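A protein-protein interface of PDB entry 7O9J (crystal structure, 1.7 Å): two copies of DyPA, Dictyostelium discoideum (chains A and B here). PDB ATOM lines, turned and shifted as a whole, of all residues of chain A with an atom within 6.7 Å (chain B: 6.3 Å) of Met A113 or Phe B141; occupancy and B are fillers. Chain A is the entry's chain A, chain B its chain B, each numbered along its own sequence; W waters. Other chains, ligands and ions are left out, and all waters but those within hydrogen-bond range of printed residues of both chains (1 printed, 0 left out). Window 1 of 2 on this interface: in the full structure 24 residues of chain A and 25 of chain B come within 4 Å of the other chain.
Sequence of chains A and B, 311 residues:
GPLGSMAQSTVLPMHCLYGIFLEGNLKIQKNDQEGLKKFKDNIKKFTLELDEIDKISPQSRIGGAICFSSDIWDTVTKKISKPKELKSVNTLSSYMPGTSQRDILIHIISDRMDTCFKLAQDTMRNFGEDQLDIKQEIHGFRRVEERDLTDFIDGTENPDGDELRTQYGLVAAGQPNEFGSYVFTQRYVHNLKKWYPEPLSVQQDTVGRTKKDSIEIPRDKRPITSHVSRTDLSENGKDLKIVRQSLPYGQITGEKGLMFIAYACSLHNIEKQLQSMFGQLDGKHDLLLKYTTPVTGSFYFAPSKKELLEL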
ATOM      1  N   TYR A  18      27.320 -22.960  -6.974  1.00  0.00           N
ATOM      2  CA  TYR A  18      27.473 -24.122  -6.112  1.00  0.00           C
ATOM      3  C   TYR A  18      26.563 -25.223  -6.621  1.00  0.00           C
ATOM      4  O   TYR A  18      25.489 -24.956  -7.170  1.00  0.00           O
ATOM      5  CB  TYR A  18      27.119 -23.811  -4.633  1.00  0.00           C
ATOM      6  CG  TYR A  18      27.963 -22.690  -4.112  1.00  0.00           C
ATOM      7  CD1 TYR A  18      29.240 -22.944  -3.617  1.00  0.00           C
ATOM      8  CD2 TYR A  18      27.539 -21.369  -4.217  1.00  0.00           C
ATOM      9  CE1 TYR A  18      30.062 -21.908  -3.205  1.00  0.00           C
ATOM     10  CE2 TYR A  18      28.350 -20.328  -3.798  1.00  0.00           C
ATOM     11  CZ  TYR A  18      29.608 -20.605  -3.293  1.00  0.00           C
ATOM     12  OH  TYR A  18      30.427 -19.568  -2.897  1.00  0.00           O
ATOM     13  N   GLY A  19      27.008 -26.463  -6.442  1.00  0.00           N
ATOM     14  CA  GLY A  19      26.140 -27.587  -6.723  1.00  0.00           C
ATOM     15  C   GLY A  19      26.458 -28.731  -5.796  1.00  0.00           C
ATOM     16  O   GLY A  19      27.631 -29.007  -5.533  1.00  0.00           O
ATOM     17  N   ILE A  20      25.440 -29.402  -5.274  1.00  0.00           N
ATOM     18  CA  ILE A  20      25.641 -30.588  -4.455  1.00  0.00           C
ATOM     19  C   ILE A  20      25.060 -31.773  -5.213  1.00  0.00           C
ATOM     20  O   ILE A  20      23.974 -31.673  -5.797  1.00  0.00           O
ATOM     21  CB  ILE A  20      25.019 -30.421  -3.057  1.00  0.00           C
ATOM     22  CG1 ILE A  20      25.817 -29.363  -2.279  1.00  0.00           C
ATOM     23  CG2 ILE A  20      25.022 -31.753  -2.300  1.00  0.00           C
ATOM     24  CD1 ILE A  20      25.185 -28.963  -0.918  1.00  0.00           C
ATOM     25  N   SER A 110      22.821 -23.669  -6.540  1.00  0.00           N
ATOM     26  CA  SER A 110      22.536 -22.434  -5.822  1.00  0.00           C
ATOM     27  C   SER A 110      23.644 -21.442  -6.130  1.00  0.00           C
ATOM     28  O   SER A 110      24.742 -21.830  -6.523  1.00  0.00           O
ATOM     29  CB  SER A 110      22.457 -22.661  -4.308  1.00  0.00           C
ATOM     30  OG  SER A 110      22.043 -21.475  -3.627  1.00  0.00           O
ATOM     31  N   ASP A 111      23.356 -20.161  -5.917  1.00  0.00           N
ATOM     32  CA  ASP A 111      24.425 -19.159  -5.898  1.00  0.00           C
ATOM     33  C   ASP A 111      24.957 -18.899  -4.488  1.00  0.00           C
ATOM     34  O   ASP A 111      25.831 -18.037  -4.318  1.00  0.00           O
ATOM     35  CB  ASP A 111      23.947 -17.840  -6.518  1.00  0.00           C
ATOM     36  CG  ASP A 111      23.873 -17.893  -8.047  1.00  0.00           C
ATOM     37  OD1 ASP A 111      24.056 -18.989  -8.636  1.00  0.00           O
ATOM     38  OD2 ASP A 111      23.645 -16.820  -8.660  1.00  0.00           O
ATOM     39  N   ARG A 112      24.460 -19.625  -3.483  1.00  0.00           N
ATOM     40  CA  ARG A 112      24.962 -19.556  -2.109  1.00  0.00           C
ATOM     41  C   ARG A 112      25.126 -20.972  -1.576  1.00  0.00           C
ATOM     42  O   ARG A 112      24.203 -21.783  -1.697  1.00  0.00           O
ATOM     43  CB  ARG A 112      23.991 -18.815  -1.173  1.00  0.00           C
ATOM     44  CG  ARG A 112      23.742 -17.356  -1.521  1.00  0.00           C
ATOM     45  CD  ARG A 112      22.704 -16.757  -0.572  1.00  0.00           C
ATOM     46  NE  ARG A 112      23.175 -16.813   0.817  1.00  0.00           N
ATOM     47  CZ  ARG A 112      23.886 -15.860   1.413  1.00  0.00           C
ATOM     48  NH1 ARG A 112      24.200 -14.737   0.763  1.00  0.00           N
ATOM     49  NH2 ARG A 112      24.271 -16.024   2.678  1.00  0.00           N
ATOM     50  N   MET A 113      26.263 -21.260  -0.942  1.00  0.00           N
ATOM     51  CA  MET A 113      26.415 -22.586  -0.348  1.00  0.00           C
ATOM     52  C   MET A 113      25.446 -22.803   0.809  1.00  0.00           C
ATOM     53  O   MET A 113      25.014 -23.941   1.032  1.00  0.00           O
ATOM     54  CB  MET A 113      27.862 -22.807   0.125  1.00  0.00           C
ATOM     55  CG  MET A 113      28.123 -24.177   0.767  1.00  0.00           C
ATOM     56  SD  MET A 113      27.855 -25.556  -0.376  1.00  0.00           S
ATOM     57  CE  MET A 113      28.474 -26.932   0.610  1.00  0.00           C
ATOM     58  N   ASP A 114      25.087 -21.754   1.563  1.00  0.00           N
ATOM     59  CA  ASP A 114      24.276 -22.039   2.747  1.00  0.00           C
ATOM     60  C   ASP A 114      22.903 -22.575   2.355  1.00  0.00           C
ATOM     61  O   ASP A 114      22.421 -23.543   2.960  1.00  0.00           O
ATOM     62  CB  ASP A 114      24.195 -20.829   3.707  1.00  0.00           C
ATOM     63  CG  ASP A 114      23.573 -19.558   3.102  1.00  0.00           C
ATOM     64  OD1 ASP A 114      23.148 -19.525   1.930  1.00  0.00           O
ATOM     65  OD2 ASP A 114      23.511 -18.547   3.857  1.00  0.00           O
ATOM     66  N   THR A 115      22.289 -22.030   1.299  1.00  0.00           N
ATOM     67  CA  THR A 115      20.999 -22.582   0.886  1.00  0.00           C
ATOM     68  C   THR A 115      21.146 -23.881   0.089  1.00  0.00           C
ATOM     69  O   THR A 115      20.252 -24.738   0.165  1.00  0.00           O
ATOM     70  CB  THR A 115      20.202 -21.552   0.082  1.00  0.00           C
ATOM     71  OG1 THR A 115      21.012 -21.046  -0.981  1.00  0.00           O
ATOM     72  CG2 THR A 115      19.752 -20.393   0.983  1.00  0.00           C
ATOM     73  N   CYS A 116      22.240 -24.043  -0.664  1.00  0.00           N
ATOM     74  CA  CYS A 116      22.517 -25.326  -1.310  1.00  0.00           C
ATOM     75  C   CYS A 116      22.568 -26.433  -0.264  1.00  0.00           C
ATOM     76  O   CYS A 116      21.881 -27.458  -0.374  1.00  0.00           O
ATOM     77  CB  CYS A 116      23.844 -25.235  -2.069  1.00  0.00           C
ATOM     78  SG  CYS A 116      24.027 -26.404  -3.439  1.00  0.00           S
ATOM     79  N   PHE A 117      23.337 -26.201   0.797  1.00  0.00           N
ATOM     80  CA  PHE A 117      23.528 -27.207   1.835  1.00  0.00           C
ATOM     81  C   PHE A 117      22.257 -27.438   2.640  1.00  0.00           C
ATOM     82  O   PHE A 117      21.957 -28.581   3.004  1.00  0.00           O
ATOM     83  CB  PHE A 117      24.680 -26.768   2.745  1.00  0.00           C
ATOM     84  CG  PHE A 117      25.096 -27.807   3.745  1.00  0.00           C
ATOM     85  CD1 PHE A 117      26.068 -28.744   3.425  1.00  0.00           C
ATOM     86  CD2 PHE A 117      24.512 -27.828   5.012  1.00  0.00           C
ATOM     87  CE1 PHE A 117      26.457 -29.710   4.360  1.00  0.00           C
ATOM     88  CE2 PHE A 117      24.883 -28.795   5.943  1.00  0.00           C
ATOM     89  CZ  PHE A 117      25.865 -29.732   5.612  1.00  0.00           C
ATOM     90  N   LYS A 118      21.505 -26.374   2.945  1.00  0.00           N
ATOM     91  CA  LYS A 118      20.264 -26.541   3.700  1.00  0.00           C
ATOM     92  C   LYS A 118      19.298 -27.468   2.970  1.00  0.00           C
ATOM     93  O   LYS A 118      18.740 -28.397   3.564  1.00  0.00           O
ATOM     94  CB  LYS A 118      19.606 -25.186   3.946  1.00  0.00           C
ATOM     95  CG  LYS A 118      18.156 -25.319   4.445  1.00  0.00           C
ATOM     96  CD  LYS A 118      17.600 -23.975   4.882  1.00  0.00           C
ATOM     97  CE  LYS A 118      16.106 -24.069   5.196  1.00  0.00           C
ATOM     98  NZ  LYS A 118      15.834 -25.085   6.259  1.00  0.00           N
ATOM     99  N   HIS A 139      30.553 -31.783  -3.297  1.00  0.00           N
ATOM    100  CA  HIS A 139      30.286 -30.351  -3.160  1.00  0.00           C
ATOM    101  C   HIS A 139      31.030 -29.636  -4.285  1.00  0.00           C
ATOM    102  O   HIS A 139      32.240 -29.419  -4.195  1.00  0.00           O
ATOM    103  CB  HIS A 139      30.751 -29.839  -1.799  1.00  0.00           C
ATOM    104  CG  HIS A 139      30.042 -30.473  -0.645  1.00  0.00           C
ATOM    105  ND1 HIS A 139      30.339 -30.173   0.670  1.00  0.00           N
ATOM    106  CD2 HIS A 139      29.046 -31.391  -0.611  1.00  0.00           C
ATOM    107  CE1 HIS A 139      29.552 -30.885   1.466  1.00  0.00           C
ATOM    108  NE2 HIS A 139      28.764 -31.636   0.712  1.00  0.00           N
ATOM    109  N   GLY A 140      30.317 -29.296  -5.360  1.00  0.00           N
ATOM    110  CA  GLY A 140      30.929 -28.564  -6.462  1.00  0.00           C
ATOM    111  C   GLY A 140      30.865 -27.058  -6.238  1.00  0.00           C
ATOM    112  O   GLY A 140      29.952 -26.546  -5.592  1.00  0.00           O
ATOM    113  N   CYS B  16      32.193 -13.904   7.907  1.00  0.00           N
ATOM    114  CA  CYS B  16      32.630 -14.546   6.665  1.00  0.00           C
ATOM    115  C   CYS B  16      31.723 -15.719   6.308  1.00  0.00           C
ATOM    116  O   CYS B  16      31.184 -16.406   7.176  1.00  0.00           O
ATOM    117  CB  CYS B  16      34.078 -15.038   6.807  1.00  0.00           C
ATOM    118  SG  CYS B  16      34.399 -16.278   8.104  1.00  0.00           S
ATOM    119  N   LEU B  17      31.554 -15.959   5.012  1.00  0.00           N
ATOM    120  CA  LEU B  17      30.721 -17.074   4.580  1.00  0.00           C
ATOM    121  C   LEU B  17      31.518 -18.331   4.244  1.00  0.00           C
ATOM    122  O   LEU B  17      30.929 -19.422   4.203  1.00  0.00           O
ATOM    123  CB  LEU B  17      29.873 -16.660   3.358  1.00  0.00           C
ATOM    124  CG  LEU B  17      28.940 -15.470   3.631  1.00  0.00           C
ATOM    125  CD1 LEU B  17      28.178 -15.099   2.359  1.00  0.00           C
ATOM    126  CD2 LEU B  17      27.975 -15.793   4.801  1.00  0.00           C
ATOM    127  N   TYR B  18      32.828 -18.200   3.989  1.00  0.00           N
ATOM    128  CA  TYR B  18      33.693 -19.316   3.633  1.00  0.00           C
ATOM    129  C   TYR B  18      35.020 -19.150   4.355  1.00  0.00           C
ATOM    130  O   TYR B  18      35.465 -18.031   4.612  1.00  0.00           O
ATOM    131  CB  TYR B  18      33.941 -19.400   2.103  1.00  0.00           C
ATOM    132  CG  TYR B  18      32.644 -19.482   1.370  1.00  0.00           C
ATOM    133  CD1 TYR B  18      32.035 -20.713   1.166  1.00  0.00           C
ATOM    134  CD2 TYR B  18      31.979 -18.328   0.952  1.00  0.00           C
ATOM    135  CE1 TYR B  18      30.808 -20.808   0.553  1.00  0.00           C
ATOM    136  CE2 TYR B  18      30.752 -18.413   0.325  1.00  0.00           C
ATOM    137  CZ  TYR B  18      30.173 -19.659   0.131  1.00  0.00           C
ATOM    138  OH  TYR B  18      28.944 -19.762  -0.475  1.00  0.00           O
ATOM    139  N   GLY B  19      35.663 -20.277   4.665  1.00  0.00           N
ATOM    140  CA  GLY B  19      37.003 -20.206   5.221  1.00  0.00           C
ATOM    141  C   GLY B  19      37.791 -21.422   4.790  1.00  0.00           C
ATOM    142  O   GLY B  19      37.243 -22.522   4.800  1.00  0.00           O
ATOM    143  N   HIS B 139      37.640 -27.090   4.150  1.00  0.00           N
ATOM    144  CA  HIS B 139      36.809 -26.081   3.491  1.00  0.00           C
ATOM    145  C   HIS B 139      35.625 -25.816   4.409  1.00  0.00           C
ATOM    146  O   HIS B 139      34.685 -26.613   4.473  1.00  0.00           O
ATOM    147  CB  HIS B 139      36.337 -26.558   2.122  1.00  0.00           C
ATOM    148  CG  HIS B 139      37.453 -26.815   1.160  1.00  0.00           C
ATOM    149  ND1 HIS B 139      37.247 -27.356  -0.091  1.00  0.00           N
ATOM    150  CD2 HIS B 139      38.791 -26.634   1.281  1.00  0.00           C
ATOM    151  CE1 HIS B 139      38.410 -27.475  -0.714  1.00  0.00           C
ATOM    152  NE2 HIS B 139      39.363 -27.041   0.093  1.00  0.00           N
ATOM    153  N   GLY B 140      35.659 -24.697   5.128  1.00  0.00           N
ATOM    154  CA  GLY B 140      34.559 -24.352   6.012  1.00  0.00           C
ATOM    155  C   GLY B 140      33.541 -23.484   5.293  1.00  0.00           C
ATOM    156  O   GLY B 140      33.873 -22.759   4.355  1.00  0.00           O
ATOM    157  N   PHE B 141      32.281 -23.576   5.720  1.00  0.00           N
ATOM    158  CA  PHE B 141      31.240 -22.750   5.123  1.00  0.00           C
ATOM    159  C   PHE B 141      30.190 -22.396   6.173  1.00  0.00           C
ATOM    160  O   PHE B 141      29.842 -23.219   7.035  1.00  0.00           O
ATOM    161  CB  PHE B 141      30.591 -23.457   3.907  1.00  0.00           C
ATOM    162  CG  PHE B 141      30.039 -24.821   4.218  1.00  0.00           C
ATOM    163  CD1 PHE B 141      30.839 -25.954   4.095  1.00  0.00           C
ATOM    164  CD2 PHE B 141      28.728 -24.973   4.632  1.00  0.00           C
ATOM    165  CE1 PHE B 141      30.345 -27.214   4.381  1.00  0.00           C
ATOM    166  CE2 PHE B 141      28.229 -26.231   4.933  1.00  0.00           C
ATOM    167  CZ  PHE B 141      29.039 -27.351   4.808  1.00  0.00           C
ATOM    168  N   ARG B 142      29.691 -21.161   6.091  1.00  0.00           N
ATOM    169  CA  ARG B 142      28.622 -20.728   6.985  1.00  0.00           C
ATOM    170  C   ARG B 142      27.306 -21.370   6.562  1.00  0.00           C
ATOM    171  O   ARG B 142      27.025 -21.514   5.369  1.00  0.00           O
ATOM    172  CB  ARG B 142      28.493 -19.200   6.957  1.00  0.00           C
ATOM    173  CG  ARG B 142      27.636 -18.630   8.110  1.00  0.00           C
ATOM    174  CD  ARG B 142      28.432 -18.571   9.409  1.00  0.00           C
ATOM    175  NE  ARG B 142      29.554 -17.632   9.312  1.00  0.00           N
ATOM    176  CZ  ARG B 142      30.350 -17.310  10.327  1.00  0.00           C
ATOM    177  NH1 ARG B 142      30.130 -17.827  11.531  1.00  0.00           N
ATOM    178  NH2 ARG B 142      31.362 -16.458  10.147  1.00  0.00           N
ATOM    179  N   ARG B 143      26.491 -21.749   7.542  1.00  0.00           N
ATOM    180  CA  ARG B 143      25.170 -22.294   7.273  1.00  0.00           C
ATOM    181  C   ARG B 143      24.100 -21.226   7.483  1.00  0.00           C
ATOM    182  O   ARG B 143      24.352 -20.137   8.019  1.00  0.00           O
ATOM    183  CB  ARG B 143      24.908 -23.523   8.160  1.00  0.00           C
ATOM    184  CG  ARG B 143      25.600 -24.780   7.621  1.00  0.00           C
ATOM    185  CD  ARG B 143      25.522 -25.936   8.613  1.00  0.00           C
ATOM    186  NE  ARG B 143      24.211 -26.577   8.656  1.00  0.00           N
ATOM    187  CZ  ARG B 143      23.430 -26.630   9.732  1.00  0.00           C
ATOM    188  NH1 ARG B 143      23.796 -26.017  10.852  1.00  0.00           N
ATOM    189  NH2 ARG B 143      22.275 -27.289   9.681  1.00  0.00           N
ATOM    190  N   LEU B 149      26.395 -27.234  13.222  1.00  0.00           N
ATOM    191  CA  LEU B 149      25.657 -28.447  12.861  1.00  0.00           C
ATOM    192  C   LEU B 149      24.859 -29.048  14.028  1.00  0.00           C
ATOM    193  O   LEU B 149      23.986 -29.893  13.783  1.00  0.00           O
ATOM    194  CB  LEU B 149      26.632 -29.474  12.265  1.00  0.00           C
ATOM    195  CG  LEU B 149      26.957 -29.156  10.797  1.00  0.00           C
ATOM    196  CD1 LEU B 149      28.214 -29.882  10.334  1.00  0.00           C
ATOM    197  CD2 LEU B 149      25.752 -29.527   9.899  1.00  0.00           C
ATOM    198  N   LEU B 247      33.909 -22.291  11.621  1.00  0.00           N
ATOM    199  CA  LEU B 247      32.916 -22.576  10.586  1.00  0.00           C
ATOM    200  C   LEU B 247      32.591 -24.059  10.547  1.00  0.00           C
ATOM    201  O   LEU B 247      33.475 -24.901  10.759  1.00  0.00           O
ATOM    202  CB  LEU B 247      33.398 -22.158   9.182  1.00  0.00           C
ATOM    203  CG  LEU B 247      33.513 -20.655   8.925  1.00  0.00           C
ATOM    204  CD1 LEU B 247      34.102 -20.432   7.532  1.00  0.00           C
ATOM    205  CD2 LEU B 247      32.147 -19.992   9.004  1.00  0.00           C
ATOM    206  N   PRO B 248      31.336 -24.408  10.250  1.00  0.00           N
ATOM    207  CA  PRO B 248      31.001 -25.796   9.900  1.00  0.00           C
ATOM    208  C   PRO B 248      31.821 -26.313   8.720  1.00  0.00           C
ATOM    209  O   PRO B 248      32.289 -25.558   7.865  1.00  0.00           O
ATOM    210  CB  PRO B 248      29.514 -25.714   9.525  1.00  0.00           C
ATOM    211  CG  PRO B 248      28.993 -24.509  10.267  1.00  0.00           C
ATOM    212  CD  PRO B 248      30.151 -23.527  10.250  1.00  0.00           C
ATOM    213  N   TYR B 249      31.949 -27.640   8.658  1.00  0.00           N
ATOM    214  CA  TYR B 249      32.569 -28.303   7.508  1.00  0.00           C
ATOM    215  C   TYR B 249      31.986 -29.709   7.400  1.00  0.00           C
ATOM    216  O   TYR B 249      31.435 -30.245   8.366  1.00  0.00           O
ATOM    217  CB  TYR B 249      34.106 -28.387   7.646  1.00  0.00           C
ATOM    218  CG  TYR B 249      34.488 -29.465   8.622  1.00  0.00           C
ATOM    219  CD1 TYR B 249      34.487 -29.211   9.996  1.00  0.00           C
ATOM    220  CD2 TYR B 249      34.776 -30.761   8.193  1.00  0.00           C
ATOM    221  CE1 TYR B 249      34.775 -30.226  10.914  1.00  0.00           C
ATOM    222  CE2 TYR B 249      35.062 -31.772   9.097  1.00  0.00           C
ATOM    223  CZ  TYR B 249      35.062 -31.496  10.453  1.00  0.00           C
ATOM    224  OH  TYR B 249      35.346 -32.506  11.338  1.00  0.00           O
ATOM    225  N   GLY B 250      32.137 -30.317   6.228  1.00  0.00           N
ATOM    226  CA  GLY B 250      32.026 -31.764   6.111  1.00  0.00           C
ATOM    227  C   GLY B 250      30.882 -32.226   5.227  1.00  0.00           C
ATOM    228  O   GLY B 250      30.216 -31.441   4.546  1.00  0.00           O
HETATM  229  O   HOH W   1      25.015 -18.112   6.092  1.00  0.00           O
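Among the printed residues, pairs that only touch across the chains: Met A113 with Phe B141, Asp A114 with Arg B142, Asp A114 with Arg B143, Phe A117 with Phe B141, Phe A117 with Arg B143 and His A139 with Gly B250.
Of the printed residues of chain B, Met A113 touches Tyr B18 (3.1 Å) and Phe B141 (3.99 Å). Of the printed residues of chain A, Phe B141 touches Met A113 and Phe A117. Of the printed residues of chain B, Tyr A18 touches Tyr B18 (2.8 Å). Of the printed residues of chain A, Arg B143 touches Asp A114 (3.8 Å) and Phe A117 (3.6 Å). Printed residues of chain B within 4 Å of Phe A117: Phe B141 (3.5 Å) and Arg B143 (3.6 Å). Of the printed residues of chain A, Arg B142 touches Asp A114. Cys A116 touches none of the printed residues of chain B. The nearest printed residue of chain B that does not touch Met A113 is Arg B142 (5.0 Å).
Water W1 bridges the side-chain carboxylate of Asp A114 and the backbone carbonyl oxygen of Arg B143.
OH of Tyr B18 lies within hydrogen-bond range of OH of Tyr A18 (2.8 Å). OH of Tyr B18 is in hydrogen-bond range of N of Met A113 (3.1 Å).
The backbone carbonyl oxygen of Cys B16 is in hydrogen-bond range of the guanidinium group of Arg B142 (3.0 Å). The side-chain carboxylate (OD2) of Asp A114 is in salt-bridge range of the guanidinium group (NH2) of Arg A112 (2.9 Å). O of Leu B17 sits at hydrogen-bond distance from N of Arg B142. The backbone carbonyl oxygen (O) of Pro B248 is in hydrogen-bond range of the backbone NH (N) of Phe B141. O of Ser A110 lies within hydrogen-bond range of N of Tyr A18 (2.9 Å).
Tyr A18 touches its own counterpart, Tyr B18. Positions printed for both chains: 18, 19, 139 and 140. Of the 8 pairs that touch across the chains among the printed residues, 1 has its exchanged pair printed and touching as well.
Hydrophobic or aromatic side chains of chain B within 4 Å of the printed part of chain A: Tyr B18 and Phe B141. Hydrophobic or aromatic side chains of chain A within 4 Å of the printed part of chain B: Tyr A18, Met A113, Phe A117 and His A139. Among the printed residues, no Asp or Glu carboxylate lies within 4 Å of a Lys or Arg side-chain nitrogen of the other chain.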
